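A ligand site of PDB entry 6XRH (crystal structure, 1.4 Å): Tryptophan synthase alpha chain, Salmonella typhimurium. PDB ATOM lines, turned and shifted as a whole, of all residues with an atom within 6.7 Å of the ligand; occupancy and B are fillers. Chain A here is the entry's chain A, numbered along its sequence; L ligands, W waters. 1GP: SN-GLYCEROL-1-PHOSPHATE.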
ATOM      1  N   PHE A  22     -19.949 -17.265  27.723  1.00  0.00           N
ATOM      2  CA  PHE A  22     -20.423 -16.102  26.987  1.00  0.00           C
ATOM      3  C   PHE A  22     -21.664 -15.540  27.659  1.00  0.00           C
ATOM      4  O   PHE A  22     -22.545 -16.298  28.077  1.00  0.00           O
ATOM      5  CB  PHE A  22     -20.742 -16.464  25.520  1.00  0.00           C
ATOM      6  CG  PHE A  22     -21.606 -15.451  24.814  1.00  0.00           C
ATOM      7  CD1 PHE A  22     -22.976 -15.446  25.001  1.00  0.00           C
ATOM      8  CD2 PHE A  22     -21.036 -14.505  23.976  1.00  0.00           C
ATOM      9  CE1 PHE A  22     -23.769 -14.513  24.365  1.00  0.00           C
ATOM     10  CE2 PHE A  22     -21.825 -13.563  23.342  1.00  0.00           C
ATOM     11  CZ  PHE A  22     -23.192 -13.571  23.531  1.00  0.00           C
ATOM     12  N   GLU A  49     -16.138 -14.378  26.645  1.00  0.00           N
ATOM     13  CA  GLU A  49     -16.691 -13.892  25.389  1.00  0.00           C
ATOM     14  C   GLU A  49     -17.941 -13.091  25.722  1.00  0.00           C
ATOM     15  O   GLU A  49     -18.820 -13.584  26.442  1.00  0.00           O
ATOM     16  CB  GLU A  49     -17.024 -15.043  24.453  1.00  0.00           C
ATOM     17  CG  GLU A  49     -15.810 -15.759  23.912  1.00  0.00           C
ATOM     18  CD  GLU A  49     -14.907 -14.865  23.076  1.00  0.00           C
ATOM     19  OE1 GLU A  49     -15.423 -14.123  22.217  1.00  0.00           O
ATOM     20  OE2 GLU A  49     -13.669 -14.913  23.284  1.00  0.00           O
ATOM     21  N   ASP A  60     -28.021 -16.034  16.310  1.00  0.00           N
ATOM     22  CA  ASP A  60     -28.437 -16.414  17.643  1.00  0.00           C
ATOM     23  C   ASP A  60     -29.854 -16.977  17.647  1.00  0.00           C
ATOM     24  O   ASP A  60     -30.740 -16.473  16.954  1.00  0.00           O
ATOM     25  CB  ASP A  60     -28.348 -15.223  18.586  1.00  0.00           C
ATOM     26  CG  ASP A  60     -26.923 -14.893  18.953  1.00  0.00           C
ATOM     27  OD1 ASP A  60     -26.229 -15.808  19.432  1.00  0.00           O
ATOM     28  OD2 ASP A  60     -26.495 -13.741  18.742  1.00  0.00           O
ATOM     29  N   THR A  63     -32.758 -17.972  22.973  1.00  0.00           N
ATOM     30  CA  THR A  63     -32.202 -17.658  24.287  1.00  0.00           C
ATOM     31  C   THR A  63     -31.403 -16.354  24.236  1.00  0.00           C
ATOM     32  O   THR A  63     -31.641 -15.441  25.036  1.00  0.00           O
ATOM     33  CB  THR A  63     -31.325 -18.803  24.788  1.00  0.00           C
ATOM     34  OG1 THR A  63     -32.120 -19.980  24.953  1.00  0.00           O
ATOM     35  CG2 THR A  63     -30.677 -18.446  26.120  1.00  0.00           C
ATOM     36  N   ILE A  64     -30.462 -16.251  23.295  1.00  0.00           N
ATOM     37  CA  ILE A  64     -29.634 -15.058  23.209  1.00  0.00           C
ATOM     38  C   ILE A  64     -30.362 -13.895  22.555  1.00  0.00           C
ATOM     39  O   ILE A  64     -30.034 -12.727  22.838  1.00  0.00           O
ATOM     40  CB  ILE A  64     -28.268 -15.420  22.593  1.00  0.00           C
ATOM     41  CG1 ILE A  64     -27.553 -16.388  23.547  1.00  0.00           C
ATOM     42  CG2 ILE A  64     -27.444 -14.154  22.346  1.00  0.00           C
ATOM     43  CD1 ILE A  64     -26.184 -16.855  23.082  1.00  0.00           C
ATOM     44  N   LEU A 100     -17.914 -10.730  20.815  1.00  0.00           N
ATOM     45  CA  LEU A 100     -18.649 -11.314  19.701  1.00  0.00           C
ATOM     46  C   LEU A 100     -19.544 -10.215  19.184  1.00  0.00           C
ATOM     47  O   LEU A 100     -20.472  -9.788  19.876  1.00  0.00           O
ATOM     48  CB  LEU A 100     -19.465 -12.523  20.123  1.00  0.00           C
ATOM     49  CG  LEU A 100     -18.746 -13.713  20.764  1.00  0.00           C
ATOM     50  CD1 LEU A 100     -19.680 -14.920  20.768  1.00  0.00           C
ATOM     51  CD2 LEU A 100     -17.466 -14.025  20.027  1.00  0.00           C
ATOM     52  N   LEU A 127     -14.492 -11.172  17.311  1.00  0.00           N
ATOM     53  CA  LEU A 127     -15.084 -12.035  16.292  1.00  0.00           C
ATOM     54  C   LEU A 127     -16.310 -11.309  15.758  1.00  0.00           C
ATOM     55  O   LEU A 127     -17.205 -10.956  16.526  1.00  0.00           O
ATOM     56  CB  LEU A 127     -15.485 -13.378  16.914  1.00  0.00           C
ATOM     57  CG  LEU A 127     -15.823 -14.537  15.976  1.00  0.00           C
ATOM     58  CD1 LEU A 127     -15.866 -15.855  16.739  1.00  0.00           C
ATOM     59  CD2 LEU A 127     -17.138 -14.292  15.268  1.00  0.00           C
ATOM     60  N   TYR A 175     -12.222 -20.116  16.412  1.00  0.00           N
ATOM     61  CA  TYR A 175     -13.560 -20.513  16.828  1.00  0.00           C
ATOM     62  C   TYR A 175     -13.955 -21.757  16.035  1.00  0.00           C
ATOM     63  O   TYR A 175     -14.205 -21.678  14.835  1.00  0.00           O
ATOM     64  CB  TYR A 175     -14.568 -19.379  16.654  1.00  0.00           C
ATOM     65  CG  TYR A 175     -15.838 -19.570  17.472  1.00  0.00           C
ATOM     66  CD1 TYR A 175     -16.714 -20.614  17.195  1.00  0.00           C
ATOM     67  CD2 TYR A 175     -16.162 -18.709  18.512  1.00  0.00           C
ATOM     68  CE1 TYR A 175     -17.864 -20.805  17.926  1.00  0.00           C
ATOM     69  CE2 TYR A 175     -17.320 -18.886  19.249  1.00  0.00           C
ATOM     70  CZ  TYR A 175     -18.171 -19.927  18.950  1.00  0.00           C
ATOM     71  OH  TYR A 175     -19.338 -20.141  19.663  1.00  0.00           O
ATOM     72  N   ARG A 179     -21.409 -27.282  15.054  1.00  0.00           N
ATOM     73  CA  ARG A 179     -22.518 -27.704  14.221  1.00  0.00           C
ATOM     74  C   ARG A 179     -22.989 -26.509  13.418  1.00  0.00           C
ATOM     75  O   ARG A 179     -22.605 -25.367  13.684  1.00  0.00           O
ATOM     76  CB  ARG A 179     -23.662 -28.247  15.088  1.00  0.00           C
ATOM     77  CG  ARG A 179     -24.176 -27.223  16.118  1.00  0.00           C
ATOM     78  CD  ARG A 179     -25.566 -27.564  16.627  1.00  0.00           C
ATOM     79  NE  ARG A 179     -25.969 -26.710  17.741  1.00  0.00           N
ATOM     80  CZ  ARG A 179     -26.359 -25.438  17.620  1.00  0.00           C
ATOM     81  NH1 ARG A 179     -26.399 -24.865  16.418  1.00  0.00           N
ATOM     82  NH2 ARG A 179     -26.702 -24.741  18.685  1.00  0.00           N
ATOM     83  N   VAL A 182     -27.865 -21.977  14.517  1.00  0.00           N
ATOM     84  CA  VAL A 182     -27.652 -20.792  15.329  1.00  0.00           C
ATOM     85  C   VAL A 182     -27.385 -21.223  16.770  1.00  0.00           C
ATOM     86  O   VAL A 182     -27.581 -22.370  17.153  1.00  0.00           O
ATOM     87  CB  VAL A 182     -28.834 -19.809  15.229  1.00  0.00           C
ATOM     88  CG1 VAL A 182     -29.066 -19.420  13.796  1.00  0.00           C
ATOM     89  CG2 VAL A 182     -30.092 -20.420  15.817  1.00  0.00           C
ATOM     90  N   THR A 183     -26.951 -20.261  17.589  1.00  0.00           N
ATOM     91  CA  THR A 183     -26.651 -20.565  18.981  1.00  0.00           C
ATOM     92  C   THR A 183     -27.861 -21.201  19.648  1.00  0.00           C
ATOM     93  O   THR A 183     -29.012 -20.916  19.310  1.00  0.00           O
ATOM     94  CB  THR A 183     -26.271 -19.309  19.744  1.00  0.00           C
ATOM     95  OG1 THR A 183     -27.374 -18.394  19.761  1.00  0.00           O
ATOM     96  CG2 THR A 183     -25.060 -18.645  19.110  1.00  0.00           C
ATOM     97  N   GLY A 184     -27.604 -22.070  20.628  1.00  0.00           N
ATOM     98  CA  GLY A 184     -28.681 -22.722  21.335  1.00  0.00           C
ATOM     99  C   GLY A 184     -28.251 -23.940  22.120  1.00  0.00           C
ATOM    100  O   GLY A 184     -27.603 -24.837  21.573  1.00  0.00           O
ATOM    101  N   ALA A 185     -28.626 -23.992  23.395  1.00  0.00           N
ATOM    102  CA  ALA A 185     -28.184 -25.090  24.244  1.00  0.00           C
ATOM    103  C   ALA A 185     -28.905 -26.394  23.912  1.00  0.00           C
ATOM    104  O   ALA A 185     -28.332 -27.469  24.070  1.00  0.00           O
ATOM    105  CB  ALA A 185     -28.392 -24.727  25.712  1.00  0.00           C
ATOM    106  N   GLU A 186     -30.155 -26.300  23.454  1.00  0.00           N
ATOM    107  CA  GLU A 186     -30.930 -27.508  23.189  1.00  0.00           C
ATOM    108  C   GLU A 186     -30.334 -28.331  22.051  1.00  0.00           C
ATOM    109  O   GLU A 186     -30.468 -29.559  22.039  1.00  0.00           O
ATOM    110  CB  GLU A 186     -32.385 -27.154  22.862  1.00  0.00           C
ATOM    111  CG  GLU A 186     -33.160 -26.527  24.008  1.00  0.00           C
ATOM    112  CD  GLU A 186     -32.760 -25.089  24.283  1.00  0.00           C
ATOM    113  OE1 GLU A 186     -32.385 -24.376  23.316  1.00  0.00           O
ATOM    114  OE2 GLU A 186     -32.799 -24.662  25.460  1.00  0.00           O
ATOM    115  N   ASN A 187     -29.671 -27.672  21.099  1.00  0.00           N
ATOM    116  CA  ASN A 187     -29.102 -28.329  19.927  1.00  0.00           C
ATOM    117  C   ASN A 187     -27.638 -28.659  20.213  1.00  0.00           C
ATOM    118  O   ASN A 187     -26.798 -27.763  20.263  1.00  0.00           O
ATOM    119  CB  ASN A 187     -29.232 -27.426  18.705  1.00  0.00           C
ATOM    120  CG  ASN A 187     -28.780 -28.098  17.425  1.00  0.00           C
ATOM    121  OD1 ASN A 187     -28.223 -29.188  17.445  1.00  0.00           O
ATOM    122  ND2 ASN A 187     -29.014 -27.429  16.292  1.00  0.00           N
ATOM    123  N   GLY A 211     -17.469 -24.069  20.132  1.00  0.00           N
ATOM    124  CA  GLY A 211     -18.650 -23.368  20.590  1.00  0.00           C
ATOM    125  C   GLY A 211     -19.876 -23.736  19.777  1.00  0.00           C
ATOM    126  O   GLY A 211     -19.771 -24.226  18.645  1.00  0.00           O
ATOM    127  N   PHE A 212     -21.045 -23.467  20.369  1.00  0.00           N
ATOM    128  CA  PHE A 212     -22.384 -23.810  19.887  1.00  0.00           C
ATOM    129  C   PHE A 212     -22.862 -25.115  20.504  1.00  0.00           C
ATOM    130  O   PHE A 212     -22.264 -26.174  20.276  1.00  0.00           O
ATOM    131  CB  PHE A 212     -22.493 -23.905  18.356  1.00  0.00           C
ATOM    132  CG  PHE A 212     -22.672 -22.580  17.668  1.00  0.00           C
ATOM    133  CD1 PHE A 212     -21.921 -21.477  18.038  1.00  0.00           C
ATOM    134  CD2 PHE A 212     -23.591 -22.436  16.652  1.00  0.00           C
ATOM    135  CE1 PHE A 212     -22.088 -20.257  17.406  1.00  0.00           C
ATOM    136  CE2 PHE A 212     -23.761 -21.222  15.997  1.00  0.00           C
ATOM    137  CZ  PHE A 212     -23.004 -20.137  16.383  1.00  0.00           C
ATOM    138  N   GLY A 213     -23.939 -25.056  21.274  1.00  0.00           N
ATOM    139  CA  GLY A 213     -24.563 -26.243  21.816  1.00  0.00           C
ATOM    140  C   GLY A 213     -23.895 -26.847  23.034  1.00  0.00           C
ATOM    141  O   GLY A 213     -24.382 -27.871  23.539  1.00  0.00           O
ATOM    142  N   ILE A 214     -22.801 -26.258  23.508  1.00  0.00           N
ATOM    143  CA  ILE A 214     -22.088 -26.785  24.674  1.00  0.00           C
ATOM    144  C   ILE A 214     -22.867 -26.363  25.920  1.00  0.00           C
ATOM    145  O   ILE A 214     -22.879 -25.189  26.288  1.00  0.00           O
ATOM    146  CB  ILE A 214     -20.649 -26.256  24.737  1.00  0.00           C
ATOM    147  CG1 ILE A 214     -19.867 -26.608  23.466  1.00  0.00           C
ATOM    148  CG2 ILE A 214     -19.938 -26.794  25.970  1.00  0.00           C
ATOM    149  CD1 ILE A 214     -19.703 -28.046  23.218  1.00  0.00           C
ATOM    150  N   SER A 215     -23.494 -27.343  26.579  1.00  0.00           N
ATOM    151  CA  SER A 215     -24.308 -27.036  27.739  1.00  0.00           C
ATOM    152  C   SER A 215     -24.110 -27.997  28.908  1.00  0.00           C
ATOM    153  O   SER A 215     -24.802 -27.851  29.915  1.00  0.00           O
ATOM    154  CB  SER A 215     -25.799 -27.015  27.352  1.00  0.00           C
ATOM    155  OG  SER A 215     -26.183 -28.237  26.739  1.00  0.00           O
ATOM    156  N   ILE A 232     -16.567 -23.033  24.665  1.00  0.00           N
ATOM    157  CA  ILE A 232     -17.348 -21.832  24.921  1.00  0.00           C
ATOM    158  C   ILE A 232     -18.791 -22.261  25.158  1.00  0.00           C
ATOM    159  O   ILE A 232     -19.316 -23.102  24.434  1.00  0.00           O
ATOM    160  CB  ILE A 232     -17.284 -20.859  23.718  1.00  0.00           C
ATOM    161  CG1 ILE A 232     -15.850 -20.361  23.505  1.00  0.00           C
ATOM    162  CG2 ILE A 232     -18.225 -19.685  23.935  1.00  0.00           C
ATOM    163  CD1 ILE A 232     -15.603 -19.799  22.115  1.00  0.00           C
ATOM    164  N   SER A 233     -19.438 -21.637  26.143  1.00  0.00           N
ATOM    165  CA  SER A 233     -20.840 -21.926  26.434  1.00  0.00           C
ATOM    166  C   SER A 233     -21.556 -20.607  26.668  1.00  0.00           C
ATOM    167  O   SER A 233     -21.149 -19.821  27.541  1.00  0.00           O
ATOM    168  CB  SER A 233     -20.955 -22.823  27.675  1.00  0.00           C
ATOM    169  OG  SER A 233     -22.316 -23.100  27.973  1.00  0.00           O
ATOM    170  N   GLY A 234     -22.622 -20.374  25.899  1.00  0.00           N
ATOM    171  CA  GLY A 234     -23.371 -19.128  25.990  1.00  0.00           C
ATOM    172  C   GLY A 234     -24.809 -19.342  26.414  1.00  0.00           C
ATOM    173  O   GLY A 234     -25.191 -18.936  27.523  1.00  0.00           O
ATOM    174  N   SER A 235     -25.607 -19.983  25.561  1.00  0.00           N
ATOM    175  CA  SER A 235     -27.033 -20.136  25.854  1.00  0.00           C
ATOM    176  C   SER A 235     -27.256 -20.837  27.187  1.00  0.00           C
ATOM    177  O   SER A 235     -28.175 -20.470  27.943  1.00  0.00           O
ATOM    178  CB  SER A 235     -27.706 -20.908  24.726  1.00  0.00           C
ATOM    179  OG  SER A 235     -27.678 -20.144  23.530  1.00  0.00           O
ATOM    180  N   ALA A 236     -26.450 -21.849  27.503  1.00  0.00           N
ATOM    181  CA  ALA A 236     -26.569 -22.515  28.793  1.00  0.00           C
ATOM    182  C   ALA A 236     -26.444 -21.509  29.930  1.00  0.00           C
ATOM    183  O   ALA A 236     -27.228 -21.535  30.895  1.00  0.00           O
ATOM    184  CB  ALA A 236     -25.498 -23.596  28.927  1.00  0.00           C
ATOM    185  N   ILE A 237     -25.475 -20.598  29.840  1.00  0.00           N
ATOM    186  CA  ILE A 237     -25.291 -19.581  30.871  1.00  0.00           C
ATOM    187  C   ILE A 237     -26.474 -18.624  30.871  1.00  0.00           C
ATOM    188  O   ILE A 237     -26.974 -18.231  31.927  1.00  0.00           O
ATOM    189  CB  ILE A 237     -23.966 -18.831  30.613  1.00  0.00           C
ATOM    190  CG1 ILE A 237     -22.775 -19.786  30.650  1.00  0.00           C
ATOM    191  CG2 ILE A 237     -23.798 -17.702  31.629  1.00  0.00           C
ATOM    192  CD1 ILE A 237     -22.350 -20.172  32.028  1.00  0.00           C
ATOM    193  N   VAL A 238     -26.934 -18.241  29.686  1.00  0.00           N
ATOM    194  CA  VAL A 238     -27.971 -17.218  29.594  1.00  0.00           C
ATOM    195  C   VAL A 238     -29.290 -17.726  30.147  1.00  0.00           C
ATOM    196  O   VAL A 238     -30.066 -16.961  30.721  1.00  0.00           O
ATOM    197  CB  VAL A 238     -28.085 -16.727  28.143  1.00  0.00           C
ATOM    198  CG1 VAL A 238     -29.246 -15.769  27.998  1.00  0.00           C
ATOM    199  CG2 VAL A 238     -26.770 -16.079  27.711  1.00  0.00           C
HETATM  200  C3  1GP L   1     -21.159 -17.792  21.945  1.00  0.00           C
HETATM  201  O3  1GP L   1     -23.478 -18.180  22.373  1.00  0.00           O
HETATM  202  C2  1GP L   1     -22.375 -18.651  21.632  1.00  0.00           C
HETATM  203  O2  1GP L   1     -20.201 -17.923  20.927  1.00  0.00           O
HETATM  204  C1  1GP L   1     -22.104 -20.104  21.985  1.00  0.00           C
HETATM  205  O1P 1GP L   1     -23.160 -20.898  21.476  1.00  0.00           O
HETATM  206  O2P 1GP L   1     -25.148 -22.478  21.782  1.00  0.00           O
HETATM  207  O3P 1GP L   1     -23.629 -22.044  23.674  1.00  0.00           O
HETATM  208  O4P 1GP L   1     -25.159 -20.271  22.887  1.00  0.00           O
HETATM  209  P   1GP L   1     -24.301 -21.439  22.465  1.00  0.00           P
HETATM  210  O   HOH W   1     -21.595 -16.538  18.763  1.00  0.00           O
HETATM  211  O   HOH W   2     -25.046 -23.317  25.864  1.00  0.00           O
HETATM  212  O   HOH W   3     -23.616 -15.479  20.289  1.00  0.00           O
HETATM  213  O   HOH W   4     -21.716 -23.462  23.037  1.00  0.00           O
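Water W2 lies within hydrogen-bond range of N of Ala 236 (2.6 Å), O of Ile 214 (2.9 Å), O3P of the ligand (2.9 Å), N of Ser 235 (3.4 Å) and OG of Ser 233 (3.5 Å). Water W3 lies within hydrogen-bond range of the side-chain carboxylate of Asp 60 (2.8 Å) and an oxygen (O3) of the ligand (3.4 Å).
The backbone NH (N) of Gly 184 is in hydrogen-bond range of an oxygen (O2P) of the ligand, 2.7 Å away. An oxygen (O2) of the ligand lies within hydrogen-bond range of the side-chain hydroxyl (OH) of Tyr 175, at 2.7 Å. The side-chain hydroxyl (OG) of Ser 235 sits at hydrogen-bond distance from an oxygen (O4P) of the ligand. O2P of the ligand is in hydrogen-bond range of N of Gly 213. An oxygen (O3P) of the ligand sits at hydrogen-bond distance from the backbone NH (N) of Gly 234 (3.0 Å). The backbone NH of Ser 235 is in hydrogen-bond range of an oxygen (O4P) of the ligand (2.7 Å).
The side-chain hydroxyl of Thr 183 is in hydrogen-bond range of the side-chain carboxylate of Asp 60, 2.8 Å away. The side-chain hydroxyl (OG) of Ser 235 is in hydrogen-bond range of the backbone NH (N) of Gly 184 (3.5 Å). O of Gly 184 lies within hydrogen-bond range of NH2 of Arg 179, at 3.0 Å. The backbone NH (N) of Phe 22 lies within hydrogen-bond range of the backbone carbonyl oxygen (O) of Ser 233. OG of Ser 233 sits at hydrogen-bond distance from O of Ile 214, at 2.7 Å.
Merely in contact with the ligand: Leu 100 (3.1 Å), Ile 64 (3.1 Å), Phe 212 (3.4 Å), Thr 183 (3.5 Å), Phe 22 (3.7 Å) and Ser 233 (3.9 Å). Hydrophobic or aromatic side chains within 4 Å of the ligand: Phe 22, Ile 64, Leu 100, Tyr 175 and Phe 212. Of the 27 residues printed, 11 come within 4 Å of the ligand.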
